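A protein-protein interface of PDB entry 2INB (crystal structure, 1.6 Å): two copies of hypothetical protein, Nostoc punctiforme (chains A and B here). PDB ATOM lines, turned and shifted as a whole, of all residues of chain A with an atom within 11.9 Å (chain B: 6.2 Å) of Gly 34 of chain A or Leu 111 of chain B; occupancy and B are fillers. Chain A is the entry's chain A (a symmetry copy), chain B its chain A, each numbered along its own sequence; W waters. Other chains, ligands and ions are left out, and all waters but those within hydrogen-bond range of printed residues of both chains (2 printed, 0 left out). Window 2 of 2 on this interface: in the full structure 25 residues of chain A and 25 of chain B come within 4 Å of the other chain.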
ATOM      1  N   ILE A  30       6.181  -3.210   7.787  1.00  0.00           N
ATOM      2  CA  ILE A  30       6.245  -4.093   6.649  1.00  0.00           C
ATOM      3  C   ILE A  30       4.842  -4.620   6.355  1.00  0.00           C
ATOM      4  O   ILE A  30       4.151  -5.083   7.272  1.00  0.00           O
ATOM      5  CB  ILE A  30       7.259  -5.234   6.929  1.00  0.00           C
ATOM      6  CG1 ILE A  30       7.435  -6.133   5.702  1.00  0.00           C
ATOM      7  CG2 ILE A  30       6.840  -6.053   8.158  1.00  0.00           C
ATOM      8  CD1 ILE A  30       8.678  -6.989   5.785  1.00  0.00           C
ATOM      9  N   SER A  31       4.434  -4.503   5.087  1.00  0.00           N
ATOM     10  CA  SER A  31       3.158  -5.032   4.603  1.00  0.00           C
ATOM     11  C   SER A  31       3.440  -5.905   3.383  1.00  0.00           C
ATOM     12  O   SER A  31       4.165  -5.511   2.457  1.00  0.00           O
ATOM     13  CB  SER A  31       2.164  -3.925   4.258  1.00  0.00           C
ATOM     14  OG  SER A  31       1.920  -3.116   5.394  1.00  0.00           O
ATOM     15  N   VAL A  32       2.853  -7.085   3.374  1.00  0.00           N
ATOM     16  CA  VAL A  32       3.020  -7.952   2.242  1.00  0.00           C
ATOM     17  C   VAL A  32       1.813  -8.857   2.168  1.00  0.00           C
ATOM     18  O   VAL A  32       1.147  -9.128   3.179  1.00  0.00           O
ATOM     19  CB  VAL A  32       4.328  -8.776   2.348  1.00  0.00           C
ATOM     20  CG1 VAL A  32       4.252  -9.755   3.505  1.00  0.00           C
ATOM     21  CG2 VAL A  32       4.640  -9.477   1.024  1.00  0.00           C
ATOM     22  N   GLY A  33       1.524  -9.292   0.949  1.00  0.00           N
ATOM     23  CA  GLY A  33       0.489 -10.274   0.704  1.00  0.00           C
ATOM     24  C   GLY A  33      -0.831 -10.018   1.423  1.00  0.00           C
ATOM     25  O   GLY A  33      -1.467 -10.950   1.888  1.00  0.00           O
ATOM     26  N   GLY A  34      -1.231  -8.750   1.481  1.00  0.00           N
ATOM     27  CA  GLY A  34      -2.567  -8.386   2.009  1.00  0.00           C
ATOM     28  C   GLY A  34      -2.625  -8.181   3.514  1.00  0.00           C
ATOM     29  O   GLY A  34      -3.722  -7.957   4.054  1.00  0.00           O
ATOM     30  N   VAL A  35      -1.463  -8.281   4.187  1.00  0.00           N
ATOM     31  CA  VAL A  35      -1.361  -8.132   5.645  1.00  0.00           C
ATOM     32  C   VAL A  35      -0.357  -7.058   6.032  1.00  0.00           C
ATOM     33  O   VAL A  35       0.734  -7.025   5.491  1.00  0.00           O
ATOM     34  CB  VAL A  35      -0.907  -9.501   6.259  1.00  0.00           C
ATOM     35  CG1 VAL A  35      -0.671  -9.377   7.748  1.00  0.00           C
ATOM     36  CG2 VAL A  35      -1.941 -10.594   5.947  1.00  0.00           C
ATOM     37  N   ASN A  36      -0.709  -6.201   6.993  1.00  0.00           N
ATOM     38  CA  ASN A  36       0.270  -5.306   7.626  1.00  0.00           C
ATOM     39  C   ASN A  36       0.808  -5.932   8.905  1.00  0.00           C
ATOM     40  O   ASN A  36       0.077  -6.119   9.864  1.00  0.00           O
ATOM     41  CB  ASN A  36      -0.308  -3.930   7.964  1.00  0.00           C
ATOM     42  CG  ASN A  36       0.600  -3.130   8.929  1.00  0.00           C
ATOM     43  OD1 ASN A  36       0.120  -2.520   9.891  1.00  0.00           O
ATOM     44  ND2 ASN A  36       1.905  -3.145   8.680  1.00  0.00           N
ATOM     45  N   LEU A  37       2.095  -6.238   8.906  1.00  0.00           N
ATOM     46  CA  LEU A  37       2.733  -6.877  10.029  1.00  0.00           C
ATOM     47  C   LEU A  37       3.208  -5.801  11.014  1.00  0.00           C
ATOM     48  O   LEU A  37       2.760  -4.638  10.928  1.00  0.00           O
ATOM     49  CB  LEU A  37       3.900  -7.720   9.537  1.00  0.00           C
ATOM     50  CG  LEU A  37       3.496  -8.980   8.776  1.00  0.00           C
ATOM     51  CD1 LEU A  37       3.668  -8.810   7.264  1.00  0.00           C
ATOM     52  CD2 LEU A  37       4.373 -10.130   9.230  1.00  0.00           C
ATOM     53  N   ASN A  82       7.201 -15.450  10.641  1.00  0.00           N
ATOM     54  CA  ASN A  82       6.400 -14.607   9.754  1.00  0.00           C
ATOM     55  C   ASN A  82       7.147 -13.349   9.323  1.00  0.00           C
ATOM     56  O   ASN A  82       7.098 -12.986   8.127  1.00  0.00           O
ATOM     57  CB  ASN A  82       5.075 -14.278  10.416  1.00  0.00           C
ATOM     58  CG  ASN A  82       4.099 -15.422  10.377  1.00  0.00           C
ATOM     59  OD1 ASN A  82       4.133 -16.251   9.475  1.00  0.00           O
ATOM     60  ND2 ASN A  82       3.178 -15.440  11.354  1.00  0.00           N
ATOM     61  N   GLY A  85       9.715 -14.339   6.731  1.00  0.00           N
ATOM     62  CA  GLY A  85       9.075 -14.540   5.408  1.00  0.00           C
ATOM     63  C   GLY A  85       8.707 -13.269   4.694  1.00  0.00           C
ATOM     64  O   GLY A  85       8.979 -13.100   3.504  1.00  0.00           O
ATOM     65  N   ALA A  86       8.113 -12.337   5.451  1.00  0.00           N
ATOM     66  CA  ALA A  86       7.746 -11.020   4.920  1.00  0.00           C
ATOM     67  C   ALA A  86       8.975 -10.270   4.437  1.00  0.00           C
ATOM     68  O   ALA A  86       9.007  -9.739   3.339  1.00  0.00           O
ATOM     69  CB  ALA A  86       7.020 -10.201   5.954  1.00  0.00           C
ATOM     70  N   ARG A  89      10.560 -11.013   1.015  1.00  0.00           N
ATOM     71  CA  ARG A  89       9.828 -10.511  -0.142  1.00  0.00           C
ATOM     72  C   ARG A  89       9.870  -8.989  -0.294  1.00  0.00           C
ATOM     73  O   ARG A  89       9.354  -8.444  -1.277  1.00  0.00           O
ATOM     74  CB  ARG A  89       8.371 -10.948  -0.036  1.00  0.00           C
ATOM     75  CG  ARG A  89       8.182 -12.458   0.088  1.00  0.00           C
ATOM     76  CD  ARG A  89       8.850 -13.259  -1.034  1.00  0.00           C
ATOM     77  NE  ARG A  89       8.578 -14.700  -0.909  1.00  0.00           N
ATOM     78  CZ  ARG A  89       7.498 -15.319  -1.380  1.00  0.00           C
ATOM     79  NH1 ARG A  89       6.540 -14.647  -2.010  1.00  0.00           N
ATOM     80  NH2 ARG A  89       7.344 -16.625  -1.205  1.00  0.00           N
ATOM     81  N   ARG A  90      10.467  -8.318   0.677  1.00  0.00           N
ATOM     82  CA  ARG A  90      10.558  -6.850   0.664  1.00  0.00           C
ATOM     83  C   ARG A  90      11.986  -6.329   0.765  1.00  0.00           C
ATOM     84  O   ARG A  90      12.357  -5.403   0.016  1.00  0.00           O
ATOM     85  CB  ARG A  90       9.781  -6.296   1.855  1.00  0.00           C
ATOM     86  CG  ARG A  90       8.319  -6.434   1.759  1.00  0.00           C
ATOM     87  CD  ARG A  90       7.818  -5.604   0.610  1.00  0.00           C
ATOM     88  NE  ARG A  90       6.376  -5.611   0.426  1.00  0.00           N
ATOM     89  CZ  ARG A  90       5.714  -6.449  -0.375  1.00  0.00           C
ATOM     90  NH1 ARG A  90       6.346  -7.400  -1.072  1.00  0.00           N
ATOM     91  NH2 ARG A  90       4.392  -6.340  -0.492  1.00  0.00           N
ATOM     92  N   THR B 107     -11.587 -15.824   4.714  1.00  0.00           N
ATOM     93  CA  THR B 107     -11.173 -14.409   4.671  1.00  0.00           C
ATOM     94  C   THR B 107      -9.674 -14.305   4.875  1.00  0.00           C
ATOM     95  O   THR B 107      -8.909 -14.280   3.903  1.00  0.00           O
ATOM     96  CB  THR B 107     -11.933 -13.574   5.736  1.00  0.00           C
ATOM     97  OG1 THR B 107     -11.794 -14.168   7.030  1.00  0.00           O
ATOM     98  CG2 THR B 107     -13.447 -13.490   5.378  1.00  0.00           C
ATOM     99  N   PHE B 108      -9.229 -14.341   6.141  1.00  0.00           N
ATOM    100  CA  PHE B 108      -7.787 -14.217   6.452  1.00  0.00           C
ATOM    101  C   PHE B 108      -6.901 -15.212   5.701  1.00  0.00           C
ATOM    102  O   PHE B 108      -5.892 -14.826   5.106  1.00  0.00           O
ATOM    103  CB  PHE B 108      -7.563 -14.357   7.960  1.00  0.00           C
ATOM    104  CG  PHE B 108      -6.125 -14.257   8.390  1.00  0.00           C
ATOM    105  CD1 PHE B 108      -5.484 -13.015   8.369  1.00  0.00           C
ATOM    106  CD2 PHE B 108      -5.431 -15.345   8.867  1.00  0.00           C
ATOM    107  CE1 PHE B 108      -4.194 -12.888   8.785  1.00  0.00           C
ATOM    108  CE2 PHE B 108      -4.123 -15.209   9.263  1.00  0.00           C
ATOM    109  CZ  PHE B 108      -3.514 -13.951   9.210  1.00  0.00           C
ATOM    110  N   PHE B 109      -7.287 -16.497   5.709  1.00  0.00           N
ATOM    111  CA  PHE B 109      -6.465 -17.529   5.074  1.00  0.00           C
ATOM    112  C   PHE B 109      -6.558 -17.536   3.551  1.00  0.00           C
ATOM    113  O   PHE B 109      -5.834 -18.296   2.916  1.00  0.00           O
ATOM    114  CB  PHE B 109      -6.694 -18.940   5.695  1.00  0.00           C
ATOM    115  CG  PHE B 109      -6.107 -19.073   7.061  1.00  0.00           C
ATOM    116  CD1 PHE B 109      -4.732 -19.136   7.207  1.00  0.00           C
ATOM    117  CD2 PHE B 109      -6.890 -18.958   8.192  1.00  0.00           C
ATOM    118  CE1 PHE B 109      -4.159 -19.192   8.462  1.00  0.00           C
ATOM    119  CE2 PHE B 109      -6.300 -19.005   9.494  1.00  0.00           C
ATOM    120  CZ  PHE B 109      -4.929 -19.101   9.584  1.00  0.00           C
ATOM    121  N   GLN B 110      -7.383 -16.684   2.957  1.00  0.00           N
ATOM    122  CA  GLN B 110      -7.322 -16.478   1.511  1.00  0.00           C
ATOM    123  C   GLN B 110      -6.426 -15.311   1.091  1.00  0.00           C
ATOM    124  O   GLN B 110      -6.195 -15.089  -0.112  1.00  0.00           O
ATOM    125  CB  GLN B 110      -8.733 -16.294   0.928  1.00  0.00           C
ATOM    126  CG  GLN B 110      -9.631 -17.529   1.158  1.00  0.00           C
ATOM    127  CD  GLN B 110      -8.929 -18.834   0.789  1.00  0.00           C
ATOM    128  OE1 GLN B 110      -8.361 -18.954  -0.313  1.00  0.00           O
ATOM    129  NE2 GLN B 110      -8.911 -19.797   1.710  1.00  0.00           N
ATOM    130  N   LEU B 111      -5.931 -14.546   2.057  1.00  0.00           N
ATOM    131  CA  LEU B 111      -4.919 -13.527   1.784  1.00  0.00           C
ATOM    132  C   LEU B 111      -3.597 -14.211   1.407  1.00  0.00           C
ATOM    133  O   LEU B 111      -3.283 -15.292   1.888  1.00  0.00           O
ATOM    134  CB  LEU B 111      -4.717 -12.585   2.979  1.00  0.00           C
ATOM    135  CG  LEU B 111      -5.985 -11.780   3.370  1.00  0.00           C
ATOM    136  CD1 LEU B 111      -5.712 -11.001   4.649  1.00  0.00           C
ATOM    137  CD2 LEU B 111      -6.438 -10.821   2.249  1.00  0.00           C
ATOM    138  N   ASP B 112      -2.832 -13.573   0.539  1.00  0.00           N
ATOM    139  CA  ASP B 112      -1.639 -14.200  -0.003  1.00  0.00           C
ATOM    140  C   ASP B 112      -0.623 -14.542   1.124  1.00  0.00           C
ATOM    141  O   ASP B 112      -0.015 -15.614   1.118  1.00  0.00           O
ATOM    142  CB  ASP B 112      -0.973 -13.314  -1.042  1.00  0.00           C
ATOM    143  CG  ASP B 112      -1.677 -13.282  -2.395  1.00  0.00           C
ATOM    144  OD1 ASP B 112      -2.589 -14.078  -2.636  1.00  0.00           O
ATOM    145  OD2 ASP B 112      -1.220 -12.441  -3.216  1.00  0.00           O
ATOM    146  N   PHE B 113      -0.434 -13.640   2.098  1.00  0.00           N
ATOM    147  CA  PHE B 113       0.624 -13.854   3.077  1.00  0.00           C
ATOM    148  C   PHE B 113       0.370 -15.084   3.969  1.00  0.00           C
ATOM    149  O   PHE B 113       1.196 -16.011   4.049  1.00  0.00           O
ATOM    150  CB  PHE B 113       0.889 -12.599   3.904  1.00  0.00           C
ATOM    151  CG  PHE B 113       1.958 -12.785   4.922  1.00  0.00           C
ATOM    152  CD1 PHE B 113       3.266 -12.821   4.534  1.00  0.00           C
ATOM    153  CD2 PHE B 113       1.647 -12.990   6.240  1.00  0.00           C
ATOM    154  CE1 PHE B 113       4.276 -13.072   5.489  1.00  0.00           C
ATOM    155  CE2 PHE B 113       2.638 -13.222   7.175  1.00  0.00           C
ATOM    156  CZ  PHE B 113       3.945 -13.217   6.822  1.00  0.00           C
ATOM    157  N   PRO B 114      -0.799 -15.138   4.656  1.00  0.00           N
ATOM    158  CA  PRO B 114      -1.046 -16.331   5.479  1.00  0.00           C
ATOM    159  C   PRO B 114      -1.064 -17.615   4.642  1.00  0.00           C
ATOM    160  O   PRO B 114      -0.583 -18.657   5.090  1.00  0.00           O
ATOM    161  CB  PRO B 114      -2.421 -16.078   6.100  1.00  0.00           C
ATOM    162  CG  PRO B 114      -2.723 -14.691   5.868  1.00  0.00           C
ATOM    163  CD  PRO B 114      -1.873 -14.142   4.814  1.00  0.00           C
ATOM    164  N   LYS B 115      -1.636 -17.571   3.450  1.00  0.00           N
ATOM    165  CA  LYS B 115      -1.656 -18.763   2.599  1.00  0.00           C
ATOM    166  C   LYS B 115      -0.219 -19.254   2.357  1.00  0.00           C
ATOM    167  O   LYS B 115       0.096 -20.474   2.465  1.00  0.00           O
ATOM    168  CB  LYS B 115      -2.358 -18.394   1.278  1.00  0.00           C
ATOM    169  CG  LYS B 115      -2.414 -19.474   0.296  1.00  0.00           C
ATOM    170  CD  LYS B 115      -3.310 -19.083  -0.915  1.00  0.00           C
ATOM    171  CE  LYS B 115      -4.749 -18.902  -0.557  1.00  0.00           C
ATOM    172  N   GLU B 116       0.662 -18.307   2.065  1.00  0.00           N
ATOM    173  CA  GLU B 116       2.090 -18.632   1.816  1.00  0.00           C
ATOM    174  C   GLU B 116       2.751 -19.220   3.050  1.00  0.00           C
ATOM    175  O   GLU B 116       3.485 -20.225   2.993  1.00  0.00           O
ATOM    176  CB  GLU B 116       2.917 -17.417   1.310  1.00  0.00           C
ATOM    177  CG  GLU B 116       4.356 -17.670   1.066  1.00  0.00           C
ATOM    178  CD  GLU B 116       4.719 -18.748   0.056  1.00  0.00           C
ATOM    179  OE1 GLU B 116       3.854 -19.143  -0.729  1.00  0.00           O
ATOM    180  OE2 GLU B 116       5.911 -19.156   0.130  1.00  0.00           O
HETATM  181  O   HOH W   1       4.728 -16.815  -2.510  1.00  0.00           O
HETATM  182  O   HOH W   2       7.694 -19.880  -2.188  1.00  0.00           O
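The backbone NH of Asp 112 of chain B is in hydrogen-bond range of the backbone carbonyl oxygen of Gly 33 of chain A (3.3 Å).
The side-chain carboxylate (OE2) of Glu 116 of chain B lies within salt-bridge range of the guanidinium group (NH2) of Arg 89 of chain A.
The backbone NH (N) of Phe 113 of chain B is in hydrogen-bond range of the backbone carbonyl oxygen (O) of Gly 33 of chain A.
N of Leu 37 of chain A is in hydrogen-bond range of O of Ile 30 of chain A.
Among the printed residues, pairs that only touch across the chains: Val 32 of chain A with Phe 113 of chain B, Asn 82 of chain A with Phe 113 of chain B, Gly 34 of chain A with Leu 111 of chain B, Val 35 of chain A with Pro 114 of chain B, Gly 33 of chain A with Leu 111 of chain B, Ala 86 of chain A with Phe 113 of chain B and Leu 37 of chain A with Phe 113 of chain B.
Of the printed residues of chain B, Val 32 of chain A touches Phe 113.
Gly 34 of chain A touches just one residue of chain B: Leu 111 (3.7 Å).
Of the printed residues of chain B, Ala 86 of chain A touches Phe 113.
No residue of chain A comes within 4 Å of Phe 108 of chain B.
Printed residues of chain A within 4 Å of Leu 111 of chain B: Gly 33 (3.8 Å) and Gly 34 (3.7 Å).
Asp 112 of chain B touches just one residue of chain A: Gly 33.
Of chain A, only Val 35 comes within 4 Å of Pro 114 of chain B.
No residue of chain A comes within 4 Å of Lys 115 of chain B.
The nearest printed residue of chain A that does not touch Leu 111 of chain B is Val 35 of chain A (4.01 Å).
Of the 10 printed residues of chain B, 5 touch a printed residue of chain A.
Printed residues of chain B that touch a printed residue of chain A: Leu 111, Asp 112, Phe 113, Pro 114 and Glu 116.
Hydrophobic or aromatic side chains of chain B within 4 Å of the printed part of chain A: Leu 111, Phe 113 and Pro 114.
Along chain B the printed residues that touch a printed residue of chain A span positions 111 to 116.
Printed residues of chain A that touch a printed residue of chain B: Val 32, Gly 33, Gly 34, Val 35, Leu 37, Asn 82, Ala 86 and Arg 89.
No position is printed for both chains.
Water W1 lies within hydrogen-bond range of NH1 of Arg 89 of chain A (2.9 Å) and OE1 of Glu 116 of chain B (3.1 Å).
Water W2 lies within hydrogen-bond range of OE2 of Glu 116 of chain B (3.0 Å) and NH2 of Arg 89 of chain A (3.4 Å).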
